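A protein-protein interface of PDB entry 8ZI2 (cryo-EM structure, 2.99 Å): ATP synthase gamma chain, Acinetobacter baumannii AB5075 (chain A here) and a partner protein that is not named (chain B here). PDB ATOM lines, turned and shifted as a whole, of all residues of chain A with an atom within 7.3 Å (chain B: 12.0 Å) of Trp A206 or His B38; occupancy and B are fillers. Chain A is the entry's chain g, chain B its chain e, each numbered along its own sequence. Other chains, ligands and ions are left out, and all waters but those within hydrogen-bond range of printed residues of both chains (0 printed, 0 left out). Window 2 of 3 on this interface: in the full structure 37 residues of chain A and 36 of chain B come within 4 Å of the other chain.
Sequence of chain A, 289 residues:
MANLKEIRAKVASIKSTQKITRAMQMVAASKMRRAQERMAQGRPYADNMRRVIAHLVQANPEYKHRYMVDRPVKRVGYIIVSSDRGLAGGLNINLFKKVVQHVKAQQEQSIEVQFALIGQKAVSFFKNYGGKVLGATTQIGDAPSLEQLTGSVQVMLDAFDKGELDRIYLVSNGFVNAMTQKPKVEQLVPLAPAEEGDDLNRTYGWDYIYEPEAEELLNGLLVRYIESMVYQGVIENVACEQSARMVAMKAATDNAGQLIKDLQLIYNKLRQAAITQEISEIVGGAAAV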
ATOM      1  N   LEU A 200     -14.684   9.827 -15.975  1.00  0.00           N
ATOM      2  CA  LEU A 200     -14.166   9.025 -14.869  1.00  0.00           C
ATOM      3  C   LEU A 200     -14.749   9.468 -13.548  1.00  0.00           C
ATOM      4  O   LEU A 200     -14.972   8.654 -12.653  1.00  0.00           O
ATOM      5  CB  LEU A 200     -12.636   9.091 -14.837  1.00  0.00           C
ATOM      6  CG  LEU A 200     -11.924   8.457 -16.036  1.00  0.00           C
ATOM      7  CD1 LEU A 200     -11.795   9.446 -17.184  1.00  0.00           C
ATOM      8  CD2 LEU A 200     -10.558   7.928 -15.633  1.00  0.00           C
ATOM      9  N   ASN A 201     -14.999  10.766 -13.422  1.00  0.00           N
ATOM     10  CA  ASN A 201     -15.637  11.294 -12.189  1.00  0.00           C
ATOM     11  C   ASN A 201     -17.014  10.643 -12.008  1.00  0.00           C
ATOM     12  O   ASN A 201     -17.206   9.954 -10.988  1.00  0.00           O
ATOM     13  CB  ASN A 201     -15.734  12.822 -12.222  1.00  0.00           C
ATOM     14  CG  ASN A 201     -16.241  13.360 -13.545  1.00  0.00           C
ATOM     15  OD1 ASN A 201     -16.452  12.605 -14.492  1.00  0.00           O
ATOM     16  ND2 ASN A 201     -16.438  14.667 -13.619  1.00  0.00           N
ATOM     17  N   ARG A 202     -17.928  10.855 -12.958  1.00  0.00           N
ATOM     18  CA  ARG A 202     -19.319  10.336 -12.829  1.00  0.00           C
ATOM     19  C   ARG A 202     -19.365   8.803 -12.858  1.00  0.00           C
ATOM     20  O   ARG A 202     -20.129   8.236 -12.054  1.00  0.00           O
ATOM     21  CB  ARG A 202     -20.193  10.920 -13.943  1.00  0.00           C
ATOM     22  CG  ARG A 202     -19.570  10.842 -15.330  1.00  0.00           C
ATOM     23  CD  ARG A 202     -20.454  11.500 -16.373  1.00  0.00           C
ATOM     24  NE  ARG A 202     -19.847  11.546 -17.695  1.00  0.00           N
ATOM     25  CZ  ARG A 202     -19.081  12.536 -18.137  1.00  0.00           C
ATOM     26  NH1 ARG A 202     -18.816  13.569 -17.355  1.00  0.00           N
ATOM     27  NH2 ARG A 202     -18.577  12.489 -19.357  1.00  0.00           N
ATOM     28  N   THR A 203     -18.609   8.150 -13.749  1.00  0.00           N
ATOM     29  CA  THR A 203     -18.744   6.671 -13.875  1.00  0.00           C
ATOM     30  C   THR A 203     -17.397   5.981 -14.099  1.00  0.00           C
ATOM     31  O   THR A 203     -16.370   6.682 -14.049  1.00  0.00           O
ATOM     32  CB  THR A 203     -19.660   6.298 -15.047  1.00  0.00           C
ATOM     33  OG1 THR A 203     -19.095   6.857 -16.233  1.00  0.00           O
ATOM     34  CG2 THR A 203     -21.083   6.787 -14.879  1.00  0.00           C
ATOM     35  N   TYR A 204     -17.406   4.653 -14.270  1.00  0.00           N
ATOM     36  CA  TYR A 204     -16.173   3.875 -14.587  1.00  0.00           C
ATOM     37  C   TYR A 204     -15.291   3.686 -13.346  1.00  0.00           C
ATOM     38  O   TYR A 204     -14.214   3.073 -13.483  1.00  0.00           O
ATOM     39  CB  TYR A 204     -15.411   4.494 -15.765  1.00  0.00           C
ATOM     40  CG  TYR A 204     -15.811   3.927 -17.102  1.00  0.00           C
ATOM     41  CD1 TYR A 204     -16.948   4.372 -17.755  1.00  0.00           C
ATOM     42  CD2 TYR A 204     -15.069   2.924 -17.702  1.00  0.00           C
ATOM     43  CE1 TYR A 204     -17.328   3.849 -18.979  1.00  0.00           C
ATOM     44  CE2 TYR A 204     -15.436   2.389 -18.925  1.00  0.00           C
ATOM     45  CZ  TYR A 204     -16.569   2.853 -19.566  1.00  0.00           C
ATOM     46  OH  TYR A 204     -16.940   2.330 -20.770  1.00  0.00           O
ATOM     47  N   GLY A 205     -15.720   4.178 -12.181  1.00  0.00           N
ATOM     48  CA  GLY A 205     -14.943   3.910 -10.956  1.00  0.00           C
ATOM     49  C   GLY A 205     -14.957   2.425 -10.649  1.00  0.00           C
ATOM     50  O   GLY A 205     -13.882   1.875 -10.341  1.00  0.00           O
ATOM     51  N   TRP A 206     -16.126   1.792 -10.774  1.00  0.00           N
ATOM     52  CA  TRP A 206     -16.264   0.335 -10.511  1.00  0.00           C
ATOM     53  C   TRP A 206     -15.631  -0.466 -11.653  1.00  0.00           C
ATOM     54  O   TRP A 206     -15.111  -1.564 -11.375  1.00  0.00           O
ATOM     55  CB  TRP A 206     -17.747  -0.014 -10.356  1.00  0.00           C
ATOM     56  CG  TRP A 206     -18.593   0.583 -11.439  1.00  0.00           C
ATOM     57  CD1 TRP A 206     -18.909   0.022 -12.642  1.00  0.00           C
ATOM     58  CD2 TRP A 206     -19.217   1.880 -11.429  1.00  0.00           C
ATOM     59  NE1 TRP A 206     -19.692   0.871 -13.374  1.00  0.00           N
ATOM     60  CE2 TRP A 206     -19.898   2.020 -12.656  1.00  0.00           C
ATOM     61  CE3 TRP A 206     -19.270   2.930 -10.505  1.00  0.00           C
ATOM     62  CZ2 TRP A 206     -20.622   3.167 -12.977  1.00  0.00           C
ATOM     63  CZ3 TRP A 206     -19.985   4.062 -10.824  1.00  0.00           C
ATOM     64  CH2 TRP A 206     -20.652   4.176 -12.043  1.00  0.00           C
ATOM     65  N   ASP A 207     -15.695   0.052 -12.884  1.00  0.00           N
ATOM     66  CA  ASP A 207     -15.180  -0.695 -14.065  1.00  0.00           C
ATOM     67  C   ASP A 207     -15.884  -2.056 -14.135  1.00  0.00           C
ATOM     68  O   ASP A 207     -17.111  -2.090 -13.919  1.00  0.00           O
ATOM     69  CB  ASP A 207     -13.653  -0.822 -14.041  1.00  0.00           C
ATOM     70  CG  ASP A 207     -12.948   0.295 -14.790  1.00  0.00           C
ATOM     71  OD1 ASP A 207     -13.624   0.994 -15.569  1.00  0.00           O
ATOM     72  OD2 ASP A 207     -11.729   0.459 -14.584  1.00  0.00           O
ATOM     73  N   TYR A 208     -15.136  -3.128 -14.414  1.00  0.00           N
ATOM     74  CA  TYR A 208     -15.739  -4.480 -14.543  1.00  0.00           C
ATOM     75  C   TYR A 208     -14.711  -5.544 -14.150  1.00  0.00           C
ATOM     76  O   TYR A 208     -13.510  -5.217 -14.088  1.00  0.00           O
ATOM     77  CB  TYR A 208     -16.209  -4.741 -15.978  1.00  0.00           C
ATOM     78  CG  TYR A 208     -16.981  -3.617 -16.622  1.00  0.00           C
ATOM     79  CD1 TYR A 208     -18.354  -3.518 -16.478  1.00  0.00           C
ATOM     80  CD2 TYR A 208     -16.339  -2.650 -17.377  1.00  0.00           C
ATOM     81  CE1 TYR A 208     -19.067  -2.486 -17.063  1.00  0.00           C
ATOM     82  CE2 TYR A 208     -17.036  -1.611 -17.969  1.00  0.00           C
ATOM     83  CZ  TYR A 208     -18.407  -1.528 -17.812  1.00  0.00           C
ATOM     84  OH  TYR A 208     -19.101  -0.508 -18.395  1.00  0.00           O
ATOM     85  N   ILE A 209     -15.149  -6.768 -13.892  1.00  0.00           N
ATOM     86  CA  ILE A 209     -14.205  -7.825 -13.570  1.00  0.00           C
ATOM     87  C   ILE A 209     -13.567  -8.362 -14.843  1.00  0.00           C
ATOM     88  O   ILE A 209     -12.488  -8.953 -14.795  1.00  0.00           O
ATOM     89  CB  ILE A 209     -14.871  -8.972 -12.790  1.00  0.00           C
ATOM     90  CG1 ILE A 209     -15.326  -8.495 -11.412  1.00  0.00           C
ATOM     91  CG2 ILE A 209     -13.913 -10.144 -12.653  1.00  0.00           C
ATOM     92  CD1 ILE A 209     -16.216  -9.491 -10.703  1.00  0.00           C
ATOM     93  N   TYR A 210     -14.230  -8.160 -15.979  1.00  0.00           N
ATOM     94  CA  TYR A 210     -13.670  -8.612 -17.245  1.00  0.00           C
ATOM     95  C   TYR A 210     -13.329 -10.078 -17.107  1.00  0.00           C
ATOM     96  O   TYR A 210     -12.246 -10.506 -17.498  1.00  0.00           O
ATOM     97  CB  TYR A 210     -12.431  -7.802 -17.619  1.00  0.00           C
ATOM     98  CG  TYR A 210     -12.615  -6.307 -17.506  1.00  0.00           C
ATOM     99  CD1 TYR A 210     -13.494  -5.630 -18.339  1.00  0.00           C
ATOM    100  CD2 TYR A 210     -11.899  -5.571 -16.572  1.00  0.00           C
ATOM    101  CE1 TYR A 210     -13.662  -4.262 -18.239  1.00  0.00           C
ATOM    102  CE2 TYR A 210     -12.059  -4.202 -16.465  1.00  0.00           C
ATOM    103  CZ  TYR A 210     -12.943  -3.554 -17.299  1.00  0.00           C
ATOM    104  OH  TYR A 210     -13.104  -2.191 -17.193  1.00  0.00           O
ATOM    105  N   LEU B  23     -34.288  -6.896 -18.854  1.00  0.00           N
ATOM    106  CA  LEU B  23     -33.097  -7.160 -19.660  1.00  0.00           C
ATOM    107  C   LEU B  23     -32.690  -8.621 -19.498  1.00  0.00           C
ATOM    108  O   LEU B  23     -31.877  -8.991 -18.647  1.00  0.00           O
ATOM    109  CB  LEU B  23     -31.965  -6.219 -19.270  1.00  0.00           C
ATOM    110  CG  LEU B  23     -31.836  -4.919 -20.067  1.00  0.00           C
ATOM    111  CD1 LEU B  23     -30.581  -4.166 -19.652  1.00  0.00           C
ATOM    112  CD2 LEU B  23     -31.830  -5.199 -21.562  1.00  0.00           C
ATOM    113  N   ALA B  28     -26.930 -14.962 -20.179  1.00  0.00           N
ATOM    114  CA  ALA B  28     -27.044 -13.800 -19.304  1.00  0.00           C
ATOM    115  C   ALA B  28     -25.923 -13.761 -18.273  1.00  0.00           C
ATOM    116  O   ALA B  28     -25.354 -12.697 -18.004  1.00  0.00           O
ATOM    117  CB  ALA B  28     -28.406 -13.796 -18.614  1.00  0.00           C
ATOM    118  N   GLY B  29     -25.590 -14.907 -17.686  1.00  0.00           N
ATOM    119  CA  GLY B  29     -24.540 -14.953 -16.691  1.00  0.00           C
ATOM    120  C   GLY B  29     -24.967 -14.619 -15.281  1.00  0.00           C
ATOM    121  O   GLY B  29     -24.104 -14.499 -14.403  1.00  0.00           O
ATOM    122  N   GLY B  30     -26.265 -14.459 -15.030  1.00  0.00           N
ATOM    123  CA  GLY B  30     -26.777 -14.234 -13.696  1.00  0.00           C
ATOM    124  C   GLY B  30     -27.051 -12.789 -13.338  1.00  0.00           C
ATOM    125  O   GLY B  30     -27.689 -12.538 -12.309  1.00  0.00           O
ATOM    126  N   GLU B  31     -26.598 -11.834 -14.149  1.00  0.00           N
ATOM    127  CA  GLU B  31     -26.855 -10.420 -13.905  1.00  0.00           C
ATOM    128  C   GLU B  31     -27.892  -9.859 -14.875  1.00  0.00           C
ATOM    129  O   GLU B  31     -27.912  -8.652 -15.140  1.00  0.00           O
ATOM    130  CB  GLU B  31     -25.551  -9.625 -13.974  1.00  0.00           C
ATOM    131  CG  GLU B  31     -24.538  -9.967 -12.887  1.00  0.00           C
ATOM    132  CD  GLU B  31     -25.086  -9.769 -11.489  1.00  0.00           C
ATOM    133  OE1 GLU B  31     -25.804  -8.772 -11.266  1.00  0.00           O
ATOM    134  OE2 GLU B  31     -24.796 -10.609 -10.612  1.00  0.00           O
ATOM    135  N   LEU B  32     -28.746 -10.721 -15.418  1.00  0.00           N
ATOM    136  CA  LEU B  32     -29.826 -10.270 -16.282  1.00  0.00           C
ATOM    137  C   LEU B  32     -30.801  -9.391 -15.510  1.00  0.00           C
ATOM    138  O   LEU B  32     -31.069  -9.621 -14.327  1.00  0.00           O
ATOM    139  CB  LEU B  32     -30.539 -11.484 -16.888  1.00  0.00           C
ATOM    140  CG  LEU B  32     -31.632 -12.237 -16.113  1.00  0.00           C
ATOM    141  CD1 LEU B  32     -33.013 -11.582 -16.174  1.00  0.00           C
ATOM    142  CD2 LEU B  32     -31.705 -13.689 -16.572  1.00  0.00           C
ATOM    143  N   GLY B  33     -31.330  -8.377 -16.184  1.00  0.00           N
ATOM    144  CA  GLY B  33     -32.328  -7.496 -15.620  1.00  0.00           C
ATOM    145  C   GLY B  33     -31.947  -6.042 -15.780  1.00  0.00           C
ATOM    146  O   GLY B  33     -30.937  -5.693 -16.387  1.00  0.00           O
ATOM    147  N   ILE B  34     -32.786  -5.178 -15.199  1.00  0.00           N
ATOM    148  CA  ILE B  34     -32.541  -3.741 -15.255  1.00  0.00           C
ATOM    149  C   ILE B  34     -31.206  -3.425 -14.579  1.00  0.00           C
ATOM    150  O   ILE B  34     -30.648  -4.237 -13.830  1.00  0.00           O
ATOM    151  CB  ILE B  34     -33.696  -2.965 -14.602  1.00  0.00           C
ATOM    152  CG1 ILE B  34     -35.038  -3.583 -14.994  1.00  0.00           C
ATOM    153  CG2 ILE B  34     -33.685  -1.502 -15.027  1.00  0.00           C
ATOM    154  CD1 ILE B  34     -35.310  -3.552 -16.485  1.00  0.00           C
ATOM    155  N   LEU B  35     -30.680  -2.227 -14.874  1.00  0.00           N
ATOM    156  CA  LEU B  35     -29.360  -1.765 -14.456  1.00  0.00           C
ATOM    157  C   LEU B  35     -29.061  -2.161 -13.013  1.00  0.00           C
ATOM    158  O   LEU B  35     -29.812  -1.811 -12.094  1.00  0.00           O
ATOM    159  CB  LEU B  35     -29.239  -0.247 -14.641  1.00  0.00           C
ATOM    160  CG  LEU B  35     -30.088   0.734 -13.820  1.00  0.00           C
ATOM    161  CD1 LEU B  35     -29.323   1.238 -12.601  1.00  0.00           C
ATOM    162  CD2 LEU B  35     -30.555   1.902 -14.669  1.00  0.00           C
ATOM    163  N   PRO B  36     -27.999  -2.932 -12.784  1.00  0.00           N
ATOM    164  CA  PRO B  36     -27.629  -3.322 -11.420  1.00  0.00           C
ATOM    165  C   PRO B  36     -26.888  -2.246 -10.641  1.00  0.00           C
ATOM    166  O   PRO B  36     -26.310  -2.555  -9.596  1.00  0.00           O
ATOM    167  CB  PRO B  36     -26.716  -4.541 -11.649  1.00  0.00           C
ATOM    168  CG  PRO B  36     -26.862  -4.897 -13.112  1.00  0.00           C
ATOM    169  CD  PRO B  36     -27.172  -3.614 -13.789  1.00  0.00           C
ATOM    170  N   GLY B  37     -26.893  -1.002 -11.119  1.00  0.00           N
ATOM    171  CA  GLY B  37     -25.992   0.015 -10.629  1.00  0.00           C
ATOM    172  C   GLY B  37     -24.615  -0.039 -11.247  1.00  0.00           C
ATOM    173  O   GLY B  37     -23.901   0.971 -11.222  1.00  0.00           O
ATOM    174  N   HIS B  38     -24.226  -1.187 -11.802  1.00  0.00           N
ATOM    175  CA  HIS B  38     -22.987  -1.359 -12.544  1.00  0.00           C
ATOM    176  C   HIS B  38     -23.015  -2.721 -13.221  1.00  0.00           C
ATOM    177  O   HIS B  38     -23.496  -3.695 -12.632  1.00  0.00           O
ATOM    178  CB  HIS B  38     -21.768  -1.240 -11.627  1.00  0.00           C
ATOM    179  CG  HIS B  38     -21.812  -2.151 -10.439  1.00  0.00           C
ATOM    180  ND1 HIS B  38     -21.687  -3.520 -10.544  1.00  0.00           N
ATOM    181  CD2 HIS B  38     -21.967  -1.889  -9.120  1.00  0.00           C
ATOM    182  CE1 HIS B  38     -21.763  -4.061  -9.341  1.00  0.00           C
ATOM    183  NE2 HIS B  38     -21.933  -3.093  -8.459  1.00  0.00           N
ATOM    184  N   ALA B  39     -22.518  -2.808 -14.449  1.00  0.00           N
ATOM    185  CA  ALA B  39     -22.468  -4.092 -15.118  1.00  0.00           C
ATOM    186  C   ALA B  39     -21.426  -4.989 -14.460  1.00  0.00           C
ATOM    187  O   ALA B  39     -20.436  -4.507 -13.905  1.00  0.00           O
ATOM    188  CB  ALA B  39     -22.145  -3.918 -16.595  1.00  0.00           C
ATOM    189  N   PRO B  40     -21.635  -6.307 -14.500  1.00  0.00           N
ATOM    190  CA  PRO B  40     -20.615  -7.203 -13.939  1.00  0.00           C
ATOM    191  C   PRO B  40     -19.355  -7.252 -14.778  1.00  0.00           C
ATOM    192  O   PRO B  40     -18.247  -7.203 -14.231  1.00  0.00           O
ATOM    193  CB  PRO B  40     -21.331  -8.560 -13.904  1.00  0.00           C
ATOM    194  CG  PRO B  40     -22.334  -8.473 -15.006  1.00  0.00           C
ATOM    195  CD  PRO B  40     -22.794  -7.042 -15.033  1.00  0.00           C
ATOM    196  N   LEU B  41     -19.500  -7.323 -16.102  1.00  0.00           N
ATOM    197  CA  LEU B  41     -18.384  -7.600 -16.996  1.00  0.00           C
ATOM    198  C   LEU B  41     -18.811  -7.499 -18.454  1.00  0.00           C
ATOM    199  O   LEU B  41     -19.978  -7.220 -18.750  1.00  0.00           O
ATOM    200  CB  LEU B  41     -17.812  -8.987 -16.685  1.00  0.00           C
ATOM    201  CG  LEU B  41     -18.809 -10.156 -16.674  1.00  0.00           C
ATOM    202  CD1 LEU B  41     -19.117 -10.715 -18.064  1.00  0.00           C
ATOM    203  CD2 LEU B  41     -18.357 -11.253 -15.723  1.00  0.00           C
ATOM    204  N   VAL B  42     -17.872  -7.716 -19.369  1.00  0.00           N
ATOM    205  CA  VAL B  42     -18.167  -7.891 -20.786  1.00  0.00           C
ATOM    206  C   VAL B  42     -17.809  -9.325 -21.155  1.00  0.00           C
ATOM    207  O   VAL B  42     -16.770  -9.843 -20.730  1.00  0.00           O
ATOM    208  CB  VAL B  42     -17.421  -6.866 -21.659  1.00  0.00           C
ATOM    209  CG1 VAL B  42     -17.764  -5.451 -21.217  1.00  0.00           C
ATOM    210  CG2 VAL B  42     -15.916  -7.085 -21.612  1.00  0.00           C
ATOM    211  N   LEU B  69     -21.752  -7.888 -25.098  1.00  0.00           N
ATOM    212  CA  LEU B  69     -22.743  -6.968 -24.476  1.00  0.00           C
ATOM    213  C   LEU B  69     -22.092  -6.153 -23.359  1.00  0.00           C
ATOM    214  O   LEU B  69     -21.417  -6.756 -22.502  1.00  0.00           O
ATOM    215  CB  LEU B  69     -23.919  -7.791 -23.939  1.00  0.00           C
ATOM    216  CG  LEU B  69     -25.112  -6.977 -23.441  1.00  0.00           C
ATOM    217  CD1 LEU B  69     -26.417  -7.715 -23.693  1.00  0.00           C
ATOM    218  CD2 LEU B  69     -24.965  -6.641 -21.965  1.00  0.00           C
ATOM    219  N   GLU B  70     -22.297  -4.833 -23.378  1.00  0.00           N
ATOM    220  CA  GLU B  70     -21.766  -3.965 -22.296  1.00  0.00           C
ATOM    221  C   GLU B  70     -22.928  -3.164 -21.705  1.00  0.00           C
ATOM    222  O   GLU B  70     -23.130  -2.012 -22.138  1.00  0.00           O
ATOM    223  CB  GLU B  70     -20.668  -3.044 -22.833  1.00  0.00           C
ATOM    224  CG  GLU B  70     -19.413  -3.784 -23.262  1.00  0.00           C
ATOM    225  CD  GLU B  70     -18.333  -2.902 -23.866  1.00  0.00           C
ATOM    226  OE1 GLU B  70     -18.620  -1.720 -24.135  1.00  0.00           O
ATOM    227  OE2 GLU B  70     -17.205  -3.399 -24.057  1.00  0.00           O
ATOM    228  N   VAL B  71     -23.689  -3.762 -20.781  1.00  0.00           N
ATOM    229  CA  VAL B  71     -24.739  -3.003 -20.121  1.00  0.00           C
ATOM    230  C   VAL B  71     -24.085  -2.003 -19.170  1.00  0.00           C
ATOM    231  O   VAL B  71     -22.890  -2.083 -18.875  1.00  0.00           O
ATOM    232  CB  VAL B  71     -25.728  -3.954 -19.399  1.00  0.00           C
ATOM    233  CG1 VAL B  71     -25.007  -4.830 -18.389  1.00  0.00           C
ATOM    234  CG2 VAL B  71     -26.908  -3.213 -18.767  1.00  0.00           C
ATOM    235  N   GLN B  72     -24.860  -1.023 -18.723  1.00  0.00           N
ATOM    236  CA  GLN B  72     -24.378   0.050 -17.865  1.00  0.00           C
ATOM    237  C   GLN B  72     -25.594   0.805 -17.351  1.00  0.00           C
ATOM    238  O   GLN B  72     -26.660   0.761 -17.978  1.00  0.00           O
ATOM    239  CB  GLN B  72     -23.446   0.997 -18.644  1.00  0.00           C
ATOM    240  CG  GLN B  72     -22.093   0.457 -19.125  1.00  0.00           C
ATOM    241  CD  GLN B  72     -21.282   1.442 -19.942  1.00  0.00           C
ATOM    242  OE1 GLN B  72     -21.834   2.351 -20.558  1.00  0.00           O
ATOM    243  NE2 GLN B  72     -19.962   1.323 -19.877  1.00  0.00           N
ATOM    244  N   PRO B  73     -25.489   1.466 -16.200  1.00  0.00           N
ATOM    245  CA  PRO B  73     -26.531   2.424 -15.821  1.00  0.00           C
ATOM    246  C   PRO B  73     -26.854   3.389 -16.949  1.00  0.00           C
ATOM    247  O   PRO B  73     -26.007   4.188 -17.360  1.00  0.00           O
ATOM    248  CB  PRO B  73     -25.915   3.140 -14.618  1.00  0.00           C
ATOM    249  CG  PRO B  73     -25.060   2.089 -13.974  1.00  0.00           C
ATOM    250  CD  PRO B  73     -24.680   1.070 -15.036  1.00  0.00           C
ATOM    251  N   HIS B  74     -28.081   3.292 -17.464  1.00  0.00           N
ATOM    252  CA  HIS B  74     -28.605   4.125 -18.543  1.00  0.00           C
ATOM    253  C   HIS B  74     -27.903   3.890 -19.876  1.00  0.00           C
ATOM    254  O   HIS B  74     -28.072   4.680 -20.810  1.00  0.00           O
ATOM    255  CB  HIS B  74     -28.549   5.614 -18.175  1.00  0.00           C
ATOM    256  CG  HIS B  74     -28.851   5.888 -16.735  1.00  0.00           C
ATOM    257  ND1 HIS B  74     -30.068   5.590 -16.159  1.00  0.00           N
ATOM    258  CD2 HIS B  74     -28.092   6.422 -15.750  1.00  0.00           C
ATOM    259  CE1 HIS B  74     -30.047   5.932 -14.884  1.00  0.00           C
ATOM    260  NE2 HIS B  74     -28.859   6.440 -14.610  1.00  0.00           N
ATOM    261  N   VAL B  75     -27.127   2.813 -20.000  1.00  0.00           N
ATOM    262  CA  VAL B  75     -26.411   2.496 -21.232  1.00  0.00           C
ATOM    263  C   VAL B  75     -26.400   0.986 -21.422  1.00  0.00           C
ATOM    264  O   VAL B  75     -25.949   0.248 -20.541  1.00  0.00           O
ATOM    265  CB  VAL B  75     -24.970   3.046 -21.216  1.00  0.00           C
ATOM    266  CG1 VAL B  75     -24.212   2.597 -22.455  1.00  0.00           C
ATOM    267  CG2 VAL B  75     -24.972   4.564 -21.114  1.00  0.00           C
ATOM    268  N   VAL B  76     -26.893   0.522 -22.568  1.00  0.00           N
ATOM    269  CA  VAL B  76     -26.811  -0.885 -22.952  1.00  0.00           C
ATOM    270  C   VAL B  76     -26.308  -0.931 -24.387  1.00  0.00           C
ATOM    271  O   VAL B  76     -26.992  -0.460 -25.305  1.00  0.00           O
ATOM    272  CB  VAL B  76     -28.156  -1.611 -22.822  1.00  0.00           C
ATOM    273  CG1 VAL B  76     -27.995  -3.083 -23.166  1.00  0.00           C
ATOM    274  CG2 VAL B  76     -28.726  -1.442 -21.423  1.00  0.00           C
ATOM    275  N   THR B  77     -25.091  -1.425 -24.580  1.00  0.00           N
ATOM    276  CA  THR B  77     -24.502  -1.435 -25.914  1.00  0.00           C
ATOM    277  C   THR B  77     -24.018  -2.819 -26.282  1.00  0.00           C
ATOM    278  O   THR B  77     -23.364  -3.487 -25.485  1.00  0.00           O
ATOM    279  CB  THR B  77     -23.315  -0.463 -26.004  1.00  0.00           C
ATOM    280  OG1 THR B  77     -22.289  -0.874 -25.093  1.00  0.00           O
ATOM    281  CG2 THR B  77     -23.757   0.950 -25.656  1.00  0.00           C
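O of Pro B40 lies within hydrogen-bond range of N of Ile A209 (3.1 Å).
OH of Tyr A204 sits at hydrogen-bond distance from NE2 of Gln B72, at 3.3 Å.
The side-chain amide nitrogen (NE2) of Gln B72 lies within hydrogen-bond range of the side-chain hydroxyl (OH) of Tyr A208 (2.5 Å).
Printed residues of chain B that touch a printed residue of chain A: His B38, Ala B39, Pro B40, Leu B41 and Gln B72.
Hydrophobic or aromatic side chains of chain B that line the printed part of chain A: His B38, Ala B39 and Leu B41.
Of the 11 printed residues of chain A, 5 touch a printed residue of chain B.
Printed residues of chain A that touch a printed residue of chain B: Tyr A204, Trp A206, Tyr A208, Ile A209 and Tyr A210.
Hydrophobic or aromatic side chains of chain A that line the printed part of chain B: Tyr A204, Trp A206 and Tyr A208.
Of the printed residues of chain B, Trp A206 touches His B38 (3.3 Å).
No residue of chain B comes within 4 Å of Asp A207.
Tyr A208 touches just these residues of chain B: Ala B39 (3.4 Å), Pro B40 (3.6 Å), Leu B41 (3.7 Å) and Gln B72 (2.5 Å).
Of the printed residues of chain B, Ile A209 touches Pro B40.
Leu B23 touches none of the printed residues of chain A.
His B38 touches just one residue of chain A: Trp A206 (3.3 Å).
Of the printed residues of chain A, Ala B39 touches Tyr A208.
Printed residues of chain A within 4 Å of Pro B40: Tyr A208 and Ile A209.
Printed residues of chain A within 4 Å of Leu B41: Tyr A208 (3.7 Å) and Tyr A210 (3.7 Å).
Among the printed residues, merely in contact across the chains: Trp A206 with His B38 (3.3 Å), Tyr A208 with Ala B39 (3.4 Å), Tyr A208 with Pro B40 (3.6 Å), Tyr A208 with Leu B41 (3.7 Å) and Tyr A210 with Leu B41 (3.7 Å).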
